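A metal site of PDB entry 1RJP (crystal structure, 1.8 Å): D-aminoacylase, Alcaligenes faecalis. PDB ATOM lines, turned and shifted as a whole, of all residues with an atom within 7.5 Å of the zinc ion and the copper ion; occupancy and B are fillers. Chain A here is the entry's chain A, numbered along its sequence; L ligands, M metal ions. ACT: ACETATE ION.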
ATOM      1  N   HIS A  80      -6.011 -25.678  19.494  1.00  0.00           N
ATOM      2  CA  HIS A  80      -6.887 -25.773  20.661  1.00  0.00           C
ATOM      3  C   HIS A  80      -8.126 -26.618  20.415  1.00  0.00           C
ATOM      4  O   HIS A  80      -9.139 -26.107  19.921  1.00  0.00           O
ATOM      5  CB  HIS A  80      -7.360 -24.390  21.098  1.00  0.00           C
ATOM      6  CG  HIS A  80      -8.018 -24.391  22.439  1.00  0.00           C
ATOM      7  ND1 HIS A  80      -7.328 -24.074  23.601  1.00  0.00           N
ATOM      8  CD2 HIS A  80      -9.243 -24.795  22.820  1.00  0.00           C
ATOM      9  CE1 HIS A  80      -8.116 -24.296  24.636  1.00  0.00           C
ATOM     10  NE2 HIS A  80      -9.283 -24.733  24.197  1.00  0.00           N
ATOM     11  N   THR A  81      -8.056 -27.905  20.752  1.00  0.00           N
ATOM     12  CA  THR A  81      -9.199 -28.774  20.539  1.00  0.00           C
ATOM     13  C   THR A  81      -9.624 -29.504  21.799  1.00  0.00           C
ATOM     14  O   THR A  81      -8.893 -29.582  22.791  1.00  0.00           O
ATOM     15  CB  THR A  81      -8.920 -29.916  19.523  1.00  0.00           C
ATOM     16  OG1 THR A  81      -8.138 -30.959  20.151  1.00  0.00           O
ATOM     17  CG2 THR A  81      -8.164 -29.402  18.328  1.00  0.00           C
ATOM     18  N   HIS A  82     -10.817 -30.054  21.703  1.00  0.00           N
ATOM     19  CA  HIS A  82     -11.372 -30.913  22.742  1.00  0.00           C
ATOM     20  C   HIS A  82     -11.779 -32.173  22.003  1.00  0.00           C
ATOM     21  O   HIS A  82     -12.866 -32.708  22.187  1.00  0.00           O
ATOM     22  CB  HIS A  82     -12.536 -30.210  23.433  1.00  0.00           C
ATOM     23  CG  HIS A  82     -12.079 -29.148  24.389  1.00  0.00           C
ATOM     24  ND1 HIS A  82     -11.382 -29.451  25.540  1.00  0.00           N
ATOM     25  CD2 HIS A  82     -12.126 -27.795  24.313  1.00  0.00           C
ATOM     26  CE1 HIS A  82     -11.017 -28.320  26.130  1.00  0.00           C
ATOM     27  NE2 HIS A  82     -11.454 -27.305  25.397  1.00  0.00           N
ATOM     28  N   GLY A 107      -6.572 -32.232  25.044  1.00  0.00           N
ATOM     29  CA  GLY A 107      -6.398 -32.107  26.491  1.00  0.00           C
ATOM     30  C   GLY A 107      -6.182 -30.680  26.970  1.00  0.00           C
ATOM     31  O   GLY A 107      -5.254 -30.405  27.760  1.00  0.00           O
ATOM     32  N   ASN A 108      -7.053 -29.785  26.514  1.00  0.00           N
ATOM     33  CA  ASN A 108      -6.970 -28.361  26.850  1.00  0.00           C
ATOM     34  C   ASN A 108      -7.843 -27.904  28.020  1.00  0.00           C
ATOM     35  O   ASN A 108      -8.772 -28.594  28.437  1.00  0.00           O
ATOM     36  CB  ASN A 108      -7.332 -27.531  25.617  1.00  0.00           C
ATOM     37  CG  ASN A 108      -6.246 -27.534  24.564  1.00  0.00           C
ATOM     38  OD1 ASN A 108      -6.283 -28.304  23.565  1.00  0.00           O
ATOM     39  ND2 ASN A 108      -5.248 -26.706  24.778  1.00  0.00           N
ATOM     40  N   CYS A 109      -7.537 -26.708  28.531  1.00  0.00           N
ATOM     41  CA  CYS A 109      -8.305 -26.082  29.605  1.00  0.00           C
ATOM     42  C   CYS A 109      -8.445 -26.908  30.881  1.00  0.00           C
ATOM     43  O   CYS A 109      -9.426 -26.762  31.633  1.00  0.00           O
ATOM     44  CB  CYS A 109      -9.678 -25.689  29.059  1.00  0.00           C
ATOM     45  SG  CYS A 109      -9.559 -24.675  27.565  1.00  0.00           S
ATOM     46  N   GLY A 110      -7.454 -27.756  31.120  1.00  0.00           N
ATOM     47  CA  GLY A 110      -7.449 -28.608  32.284  1.00  0.00           C
ATOM     48  C   GLY A 110      -8.250 -29.887  32.100  1.00  0.00           C
ATOM     49  O   GLY A 110      -8.285 -30.722  32.993  1.00  0.00           O
ATOM     50  N   ILE A 111      -8.851 -30.027  30.920  1.00  0.00           N
ATOM     51  CA  ILE A 111      -9.716 -31.161  30.584  1.00  0.00           C
ATOM     52  C   ILE A 111      -9.104 -32.214  29.651  1.00  0.00           C
ATOM     53  O   ILE A 111      -9.006 -31.969  28.453  1.00  0.00           O
ATOM     54  CB  ILE A 111     -11.006 -30.642  29.875  1.00  0.00           C
ATOM     55  CG1 ILE A 111     -11.650 -29.544  30.708  1.00  0.00           C
ATOM     56  CG2 ILE A 111     -11.990 -31.794  29.627  1.00  0.00           C
ATOM     57  CD1 ILE A 111     -12.814 -28.836  30.011  1.00  0.00           C
ATOM     58  N   LEU A 127     -17.830 -32.468  28.694  1.00  0.00           N
ATOM     59  CA  LEU A 127     -17.827 -32.038  27.281  1.00  0.00           C
ATOM     60  C   LEU A 127     -17.188 -33.114  26.378  1.00  0.00           C
ATOM     61  O   LEU A 127     -17.448 -33.136  25.183  1.00  0.00           O
ATOM     62  CB  LEU A 127     -17.075 -30.716  27.109  1.00  0.00           C
ATOM     63  CG  LEU A 127     -17.736 -29.445  27.676  1.00  0.00           C
ATOM     64  CD1 LEU A 127     -16.768 -28.304  27.488  1.00  0.00           C
ATOM     65  CD2 LEU A 127     -19.083 -29.150  26.977  1.00  0.00           C
ATOM     66  N   THR A 201      -4.357 -26.322  32.337  1.00  0.00           N
ATOM     67  CA  THR A 201      -5.142 -25.969  33.523  1.00  0.00           C
ATOM     68  C   THR A 201      -6.351 -25.119  33.063  1.00  0.00           C
ATOM     69  O   THR A 201      -6.349 -24.516  31.975  1.00  0.00           O
ATOM     70  CB  THR A 201      -4.324 -25.116  34.541  1.00  0.00           C
ATOM     71  OG1 THR A 201      -3.998 -23.862  33.941  1.00  0.00           O
ATOM     72  CG2 THR A 201      -3.034 -25.821  34.943  1.00  0.00           C
ATOM     73  N   GLY A 202      -7.391 -25.097  33.887  1.00  0.00           N
ATOM     74  CA  GLY A 202      -8.605 -24.344  33.633  1.00  0.00           C
ATOM     75  C   GLY A 202      -9.202 -23.988  34.984  1.00  0.00           C
ATOM     76  O   GLY A 202     -10.306 -24.447  35.327  1.00  0.00           O
ATOM     77  N   PHE A 204     -10.685 -21.552  35.933  1.00  0.00           N
ATOM     78  CA  PHE A 204     -11.946 -20.836  35.772  1.00  0.00           C
ATOM     79  C   PHE A 204     -13.081 -21.776  36.154  1.00  0.00           C
ATOM     80  O   PHE A 204     -14.110 -21.350  36.689  1.00  0.00           O
ATOM     81  CB  PHE A 204     -12.090 -20.434  34.300  1.00  0.00           C
ATOM     82  CG  PHE A 204     -13.470 -19.981  33.922  1.00  0.00           C
ATOM     83  CD1 PHE A 204     -13.938 -18.716  34.287  1.00  0.00           C
ATOM     84  CD2 PHE A 204     -14.292 -20.803  33.138  1.00  0.00           C
ATOM     85  CE1 PHE A 204     -15.189 -18.248  33.867  1.00  0.00           C
ATOM     86  CE2 PHE A 204     -15.562 -20.349  32.711  1.00  0.00           C
ATOM     87  CZ  PHE A 204     -16.003 -19.058  33.082  1.00  0.00           C
ATOM     88  N   TYR A 205     -12.905 -23.066  35.882  1.00  0.00           N
ATOM     89  CA  TYR A 205     -13.941 -24.056  36.135  1.00  0.00           C
ATOM     90  C   TYR A 205     -14.035 -24.629  37.560  1.00  0.00           C
ATOM     91  O   TYR A 205     -13.042 -24.720  38.295  1.00  0.00           O
ATOM     92  CB  TYR A 205     -13.810 -25.188  35.109  1.00  0.00           C
ATOM     93  CG  TYR A 205     -14.068 -24.735  33.691  1.00  0.00           C
ATOM     94  CD1 TYR A 205     -15.331 -24.300  33.283  1.00  0.00           C
ATOM     95  CD2 TYR A 205     -13.027 -24.725  32.752  1.00  0.00           C
ATOM     96  CE1 TYR A 205     -15.556 -23.867  31.967  1.00  0.00           C
ATOM     97  CE2 TYR A 205     -13.244 -24.297  31.438  1.00  0.00           C
ATOM     98  CZ  TYR A 205     -14.512 -23.881  31.055  1.00  0.00           C
ATOM     99  OH  TYR A 205     -14.725 -23.507  29.737  1.00  0.00           O
ATOM    100  N   THR A 232      -3.099 -22.860  29.246  1.00  0.00           N
ATOM    101  CA  THR A 232      -4.093 -22.452  30.211  1.00  0.00           C
ATOM    102  C   THR A 232      -5.347 -21.706  29.763  1.00  0.00           C
ATOM    103  O   THR A 232      -5.304 -20.851  28.889  1.00  0.00           O
ATOM    104  CB  THR A 232      -3.417 -21.591  31.330  1.00  0.00           C
ATOM    105  OG1 THR A 232      -4.400 -21.198  32.306  1.00  0.00           O
ATOM    106  CG2 THR A 232      -2.776 -20.311  30.735  1.00  0.00           C
ATOM    107  N   HIS A 233      -6.467 -22.083  30.364  1.00  0.00           N
ATOM    108  CA  HIS A 233      -7.705 -21.357  30.184  1.00  0.00           C
ATOM    109  C   HIS A 233      -7.542 -20.517  31.471  1.00  0.00           C
ATOM    110  O   HIS A 233      -7.686 -21.025  32.594  1.00  0.00           O
ATOM    111  CB  HIS A 233      -8.911 -22.289  30.256  1.00  0.00           C
ATOM    112  CG  HIS A 233     -10.226 -21.563  30.282  1.00  0.00           C
ATOM    113  ND1 HIS A 233     -11.352 -22.036  29.644  1.00  0.00           N
ATOM    114  CD2 HIS A 233     -10.597 -20.406  30.897  1.00  0.00           C
ATOM    115  CE1 HIS A 233     -12.357 -21.214  29.865  1.00  0.00           C
ATOM    116  NE2 HIS A 233     -11.927 -20.219  30.626  1.00  0.00           N
ATOM    117  N   MET A 234      -7.189 -19.249  31.316  1.00  0.00           N
ATOM    118  CA  MET A 234      -6.946 -18.379  32.458  1.00  0.00           C
ATOM    119  C   MET A 234      -8.078 -18.323  33.487  1.00  0.00           C
ATOM    120  O   MET A 234      -9.262 -18.520  33.176  1.00  0.00           O
ATOM    121  CB  MET A 234      -6.549 -16.985  31.966  1.00  0.00           C
ATOM    122  CG  MET A 234      -5.254 -17.027  31.132  1.00  0.00           C
ATOM    123  SD  MET A 234      -4.557 -15.373  30.797  1.00  0.00           S
ATOM    124  CE  MET A 234      -5.860 -14.628  29.791  1.00  0.00           C
ATOM    125  N   GLU A 237     -11.327 -14.154  32.407  1.00  0.00           N
ATOM    126  CA  GLU A 237     -11.072 -13.494  31.128  1.00  0.00           C
ATOM    127  C   GLU A 237     -11.887 -12.230  30.969  1.00  0.00           C
ATOM    128  O   GLU A 237     -12.160 -11.791  29.856  1.00  0.00           O
ATOM    129  CB  GLU A 237     -11.377 -14.452  29.971  1.00  0.00           C
ATOM    130  CG  GLU A 237     -10.480 -15.685  29.932  1.00  0.00           C
ATOM    131  CD  GLU A 237     -10.736 -16.554  28.702  1.00  0.00           C
ATOM    132  OE1 GLU A 237     -11.901 -16.962  28.511  1.00  0.00           O
ATOM    133  OE2 GLU A 237      -9.789 -16.823  27.930  1.00  0.00           O
ATOM    134  N   SER A 262      -4.749 -19.916  26.210  1.00  0.00           N
ATOM    135  CA  SER A 262      -5.806 -20.420  25.326  1.00  0.00           C
ATOM    136  C   SER A 262      -6.917 -19.441  25.024  1.00  0.00           C
ATOM    137  O   SER A 262      -7.260 -18.610  25.870  1.00  0.00           O
ATOM    138  CB  SER A 262      -6.435 -21.673  25.933  1.00  0.00           C
ATOM    139  OG  SER A 262      -5.475 -22.680  26.145  1.00  0.00           O
ATOM    140  N   HIS A 263      -7.495 -19.572  23.824  1.00  0.00           N
ATOM    141  CA  HIS A 263      -8.609 -18.752  23.340  1.00  0.00           C
ATOM    142  C   HIS A 263      -8.668 -17.338  23.969  1.00  0.00           C
ATOM    143  O   HIS A 263      -9.610 -16.994  24.670  1.00  0.00           O
ATOM    144  CB  HIS A 263      -9.948 -19.494  23.540  1.00  0.00           C
ATOM    145  CG  HIS A 263     -10.151 -20.068  24.920  1.00  0.00           C
ATOM    146  ND1 HIS A 263     -10.087 -19.311  26.063  1.00  0.00           N
ATOM    147  CD2 HIS A 263     -10.480 -21.329  25.325  1.00  0.00           C
ATOM    148  CE1 HIS A 263     -10.367 -20.067  27.117  1.00  0.00           C
ATOM    149  NE2 HIS A 263     -10.607 -21.296  26.694  1.00  0.00           N
ATOM    150  N   LYS A 265      -9.316 -13.594  24.803  1.00  0.00           N
ATOM    151  CA  LYS A 265     -10.482 -12.736  24.566  1.00  0.00           C
ATOM    152  C   LYS A 265     -10.629 -11.797  25.754  1.00  0.00           C
ATOM    153  O   LYS A 265      -9.933 -11.927  26.757  1.00  0.00           O
ATOM    154  CB  LYS A 265     -11.752 -13.602  24.530  1.00  0.00           C
ATOM    155  CG  LYS A 265     -12.098 -14.183  25.934  1.00  0.00           C
ATOM    156  CD  LYS A 265     -13.406 -15.019  25.974  1.00  0.00           C
ATOM    157  CE  LYS A 265     -13.286 -16.325  25.182  1.00  0.00           C
ATOM    158  NZ  LYS A 265     -12.329 -17.303  25.803  1.00  0.00           N
ATOM    159  N   TYR A 296     -10.021 -18.263  18.494  1.00  0.00           N
ATOM    160  CA  TYR A 296     -10.955 -18.690  17.455  1.00  0.00           C
ATOM    161  C   TYR A 296     -11.559 -17.396  16.873  1.00  0.00           C
ATOM    162  O   TYR A 296     -11.682 -16.390  17.566  1.00  0.00           O
ATOM    163  CB  TYR A 296     -12.022 -19.643  18.009  1.00  0.00           C
ATOM    164  CG  TYR A 296     -12.732 -19.182  19.259  1.00  0.00           C
ATOM    165  CD1 TYR A 296     -13.834 -18.323  19.198  1.00  0.00           C
ATOM    166  CD2 TYR A 296     -12.331 -19.649  20.506  1.00  0.00           C
ATOM    167  CE1 TYR A 296     -14.517 -17.954  20.353  1.00  0.00           C
ATOM    168  CE2 TYR A 296     -12.999 -19.288  21.679  1.00  0.00           C
ATOM    169  CZ  TYR A 296     -14.088 -18.439  21.592  1.00  0.00           C
ATOM    170  OH  TYR A 296     -14.724 -18.082  22.770  1.00  0.00           O
ATOM    171  N   SER A 302     -18.297 -20.936  23.976  1.00  0.00           N
ATOM    172  CA  SER A 302     -19.133 -22.088  24.229  1.00  0.00           C
ATOM    173  C   SER A 302     -18.452 -23.008  25.220  1.00  0.00           C
ATOM    174  O   SER A 302     -17.246 -23.257  25.129  1.00  0.00           O
ATOM    175  CB  SER A 302     -19.377 -22.853  22.923  1.00  0.00           C
ATOM    176  OG  SER A 302     -20.328 -23.897  23.089  1.00  0.00           O
ATOM    177  N   THR A 303     -19.219 -23.503  26.178  1.00  0.00           N
ATOM    178  CA  THR A 303     -18.704 -24.462  27.159  1.00  0.00           C
ATOM    179  C   THR A 303     -19.900 -24.957  27.959  1.00  0.00           C
ATOM    180  O   THR A 303     -21.041 -24.890  27.505  1.00  0.00           O
ATOM    181  CB  THR A 303     -17.586 -23.842  28.088  1.00  0.00           C
ATOM    182  OG1 THR A 303     -17.082 -24.834  28.987  1.00  0.00           O
ATOM    183  CG2 THR A 303     -18.122 -22.696  28.900  1.00  0.00           C
ATOM    184  N   ASP A 379     -11.431 -24.560  19.120  1.00  0.00           N
ATOM    185  CA  ASP A 379     -12.141 -24.754  20.387  1.00  0.00           C
ATOM    186  C   ASP A 379     -13.462 -25.458  20.096  1.00  0.00           C
ATOM    187  O   ASP A 379     -14.466 -25.246  20.768  1.00  0.00           O
ATOM    188  CB  ASP A 379     -12.393 -23.419  21.111  1.00  0.00           C
ATOM    189  CG  ASP A 379     -12.616 -23.599  22.621  1.00  0.00           C
ATOM    190  OD1 ASP A 379     -12.608 -24.747  23.112  1.00  0.00           O
ATOM    191  OD2 ASP A 379     -12.778 -22.592  23.330  1.00  0.00           O
ATOM    192  N   GLY A 380     -13.469 -26.309  19.065  1.00  0.00           N
ATOM    193  CA  GLY A 380     -14.686 -27.038  18.773  1.00  0.00           C
ATOM    194  C   GLY A 380     -15.054 -28.036  19.872  1.00  0.00           C
ATOM    195  O   GLY A 380     -14.182 -28.676  20.463  1.00  0.00           O
ATOM    196  N   LEU A 381     -16.341 -28.147  20.169  1.00  0.00           N
ATOM    197  CA  LEU A 381     -16.848 -29.089  21.187  1.00  0.00           C
ATOM    198  C   LEU A 381     -17.629 -30.080  20.308  1.00  0.00           C
ATOM    199  O   LEU A 381     -18.833 -29.919  20.089  1.00  0.00           O
ATOM    200  CB  LEU A 381     -17.737 -28.325  22.175  1.00  0.00           C
ATOM    201  CG  LEU A 381     -17.017 -27.095  22.748  1.00  0.00           C
ATOM    202  CD1 LEU A 381     -17.878 -26.409  23.812  1.00  0.00           C
ATOM    203  CD2 LEU A 381     -15.674 -27.513  23.353  1.00  0.00           C
ATOM    204  N   ARG A 390     -17.750 -22.861  15.076  1.00  0.00           N
ATOM    205  CA  ARG A 390     -16.284 -22.875  15.045  1.00  0.00           C
ATOM    206  C   ARG A 390     -15.811 -24.329  14.861  1.00  0.00           C
ATOM    207  O   ARG A 390     -14.740 -24.599  14.304  1.00  0.00           O
ATOM    208  CB  ARG A 390     -15.717 -22.290  16.351  1.00  0.00           C
ATOM    209  CG  ARG A 390     -16.086 -23.053  17.639  1.00  0.00           C
ATOM    210  CD  ARG A 390     -15.921 -22.166  18.890  1.00  0.00           C
ATOM    211  NE  ARG A 390     -15.876 -22.944  20.126  1.00  0.00           N
ATOM    212  CZ  ARG A 390     -15.811 -22.426  21.348  1.00  0.00           C
ATOM    213  NH1 ARG A 390     -15.774 -21.104  21.522  1.00  0.00           N
ATOM    214  NH2 ARG A 390     -15.781 -23.228  22.397  1.00  0.00           N
HETATM  215  C   ACT L   1     -13.227 -24.173  26.708  1.00  0.00           C
HETATM  216  O   ACT L   1     -12.927 -23.949  27.908  1.00  0.00           O
HETATM  217  OXT ACT L   1     -12.503 -23.828  25.749  1.00  0.00           O
HETATM  218  CH3 ACT L   1     -14.470 -24.987  26.412  1.00  0.00           C
HETATM  219 ZN    ZN M   1     -11.164 -23.007  27.799  1.00  0.00          ZN
HETATM  220 CU    CU M   2     -10.515 -25.550  25.674  1.00  0.00          CU
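The zinc ion is bound by an oxygen (O) of the ligand (2.0 Å), a ring nitrogen (ND1) of His 233 (2.1 Å), a ring nitrogen (NE2) of His 263 (2.1 Å), the side-chain sulfur of Cys 109 (2.3 Å) and an oxygen (OXT) of the ligand (2.6 Å). The zinc ion has five donor atoms within binding distance.
Within 4 Å of the zinc ion: Cys 109, His 233 and His 263. The nearest printed residue that does not touch the zinc ion is Tyr 205 (4.1 Å).
The backbone carbonyl oxygen (O) of Cys 109 sits close to the backbone NH (N) of Gly 202, at 3.5 Å. The backbone carbonyl oxygen of His 80 is in hydrogen-bond range of the backbone NH of Asp 379, at 2.9 Å. The side-chain carboxylate of Asp 379 lies within salt-bridge range of the guanidinium group of Arg 390, at 3.2 Å. The backbone carbonyl oxygen of His 263 lies within hydrogen-bond range of the side-chain amino group of Lys 265. The backbone carbonyl oxygen of Thr 81 sits close to the side-chain amide oxygen of Asn 108, 3.0 Å away. The side-chain hydroxyl (OG) of Ser 262 sits at hydrogen-bond distance from a ring nitrogen (ND1) of His 80. The side-chain carboxylate (OE2) of Glu 237 lies within hydrogen-bond range of a ring nitrogen (ND1) of His 263, 3.1 Å away. The backbone NH (N) of His 233 lies within hydrogen-bond range of the backbone carbonyl oxygen (O) of Thr 201.
Residues that only touch the copper ion: Asn 108 (3.7 Å) and Asp 379 (3.4 Å). Within 4 Å of the copper ion: His 80, His 82, Asn 108, Cys 109 and Asp 379.
A ring nitrogen (NE2) of His 82 binds the copper ion. NE2 of His 80 is bound to the copper ion, at 2.1 Å. The copper ion is bound by SG of Cys 109 (2.3 Å). Slightly farther from the copper ion lies an oxygen (OXT) of the ligand (2.6 Å).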
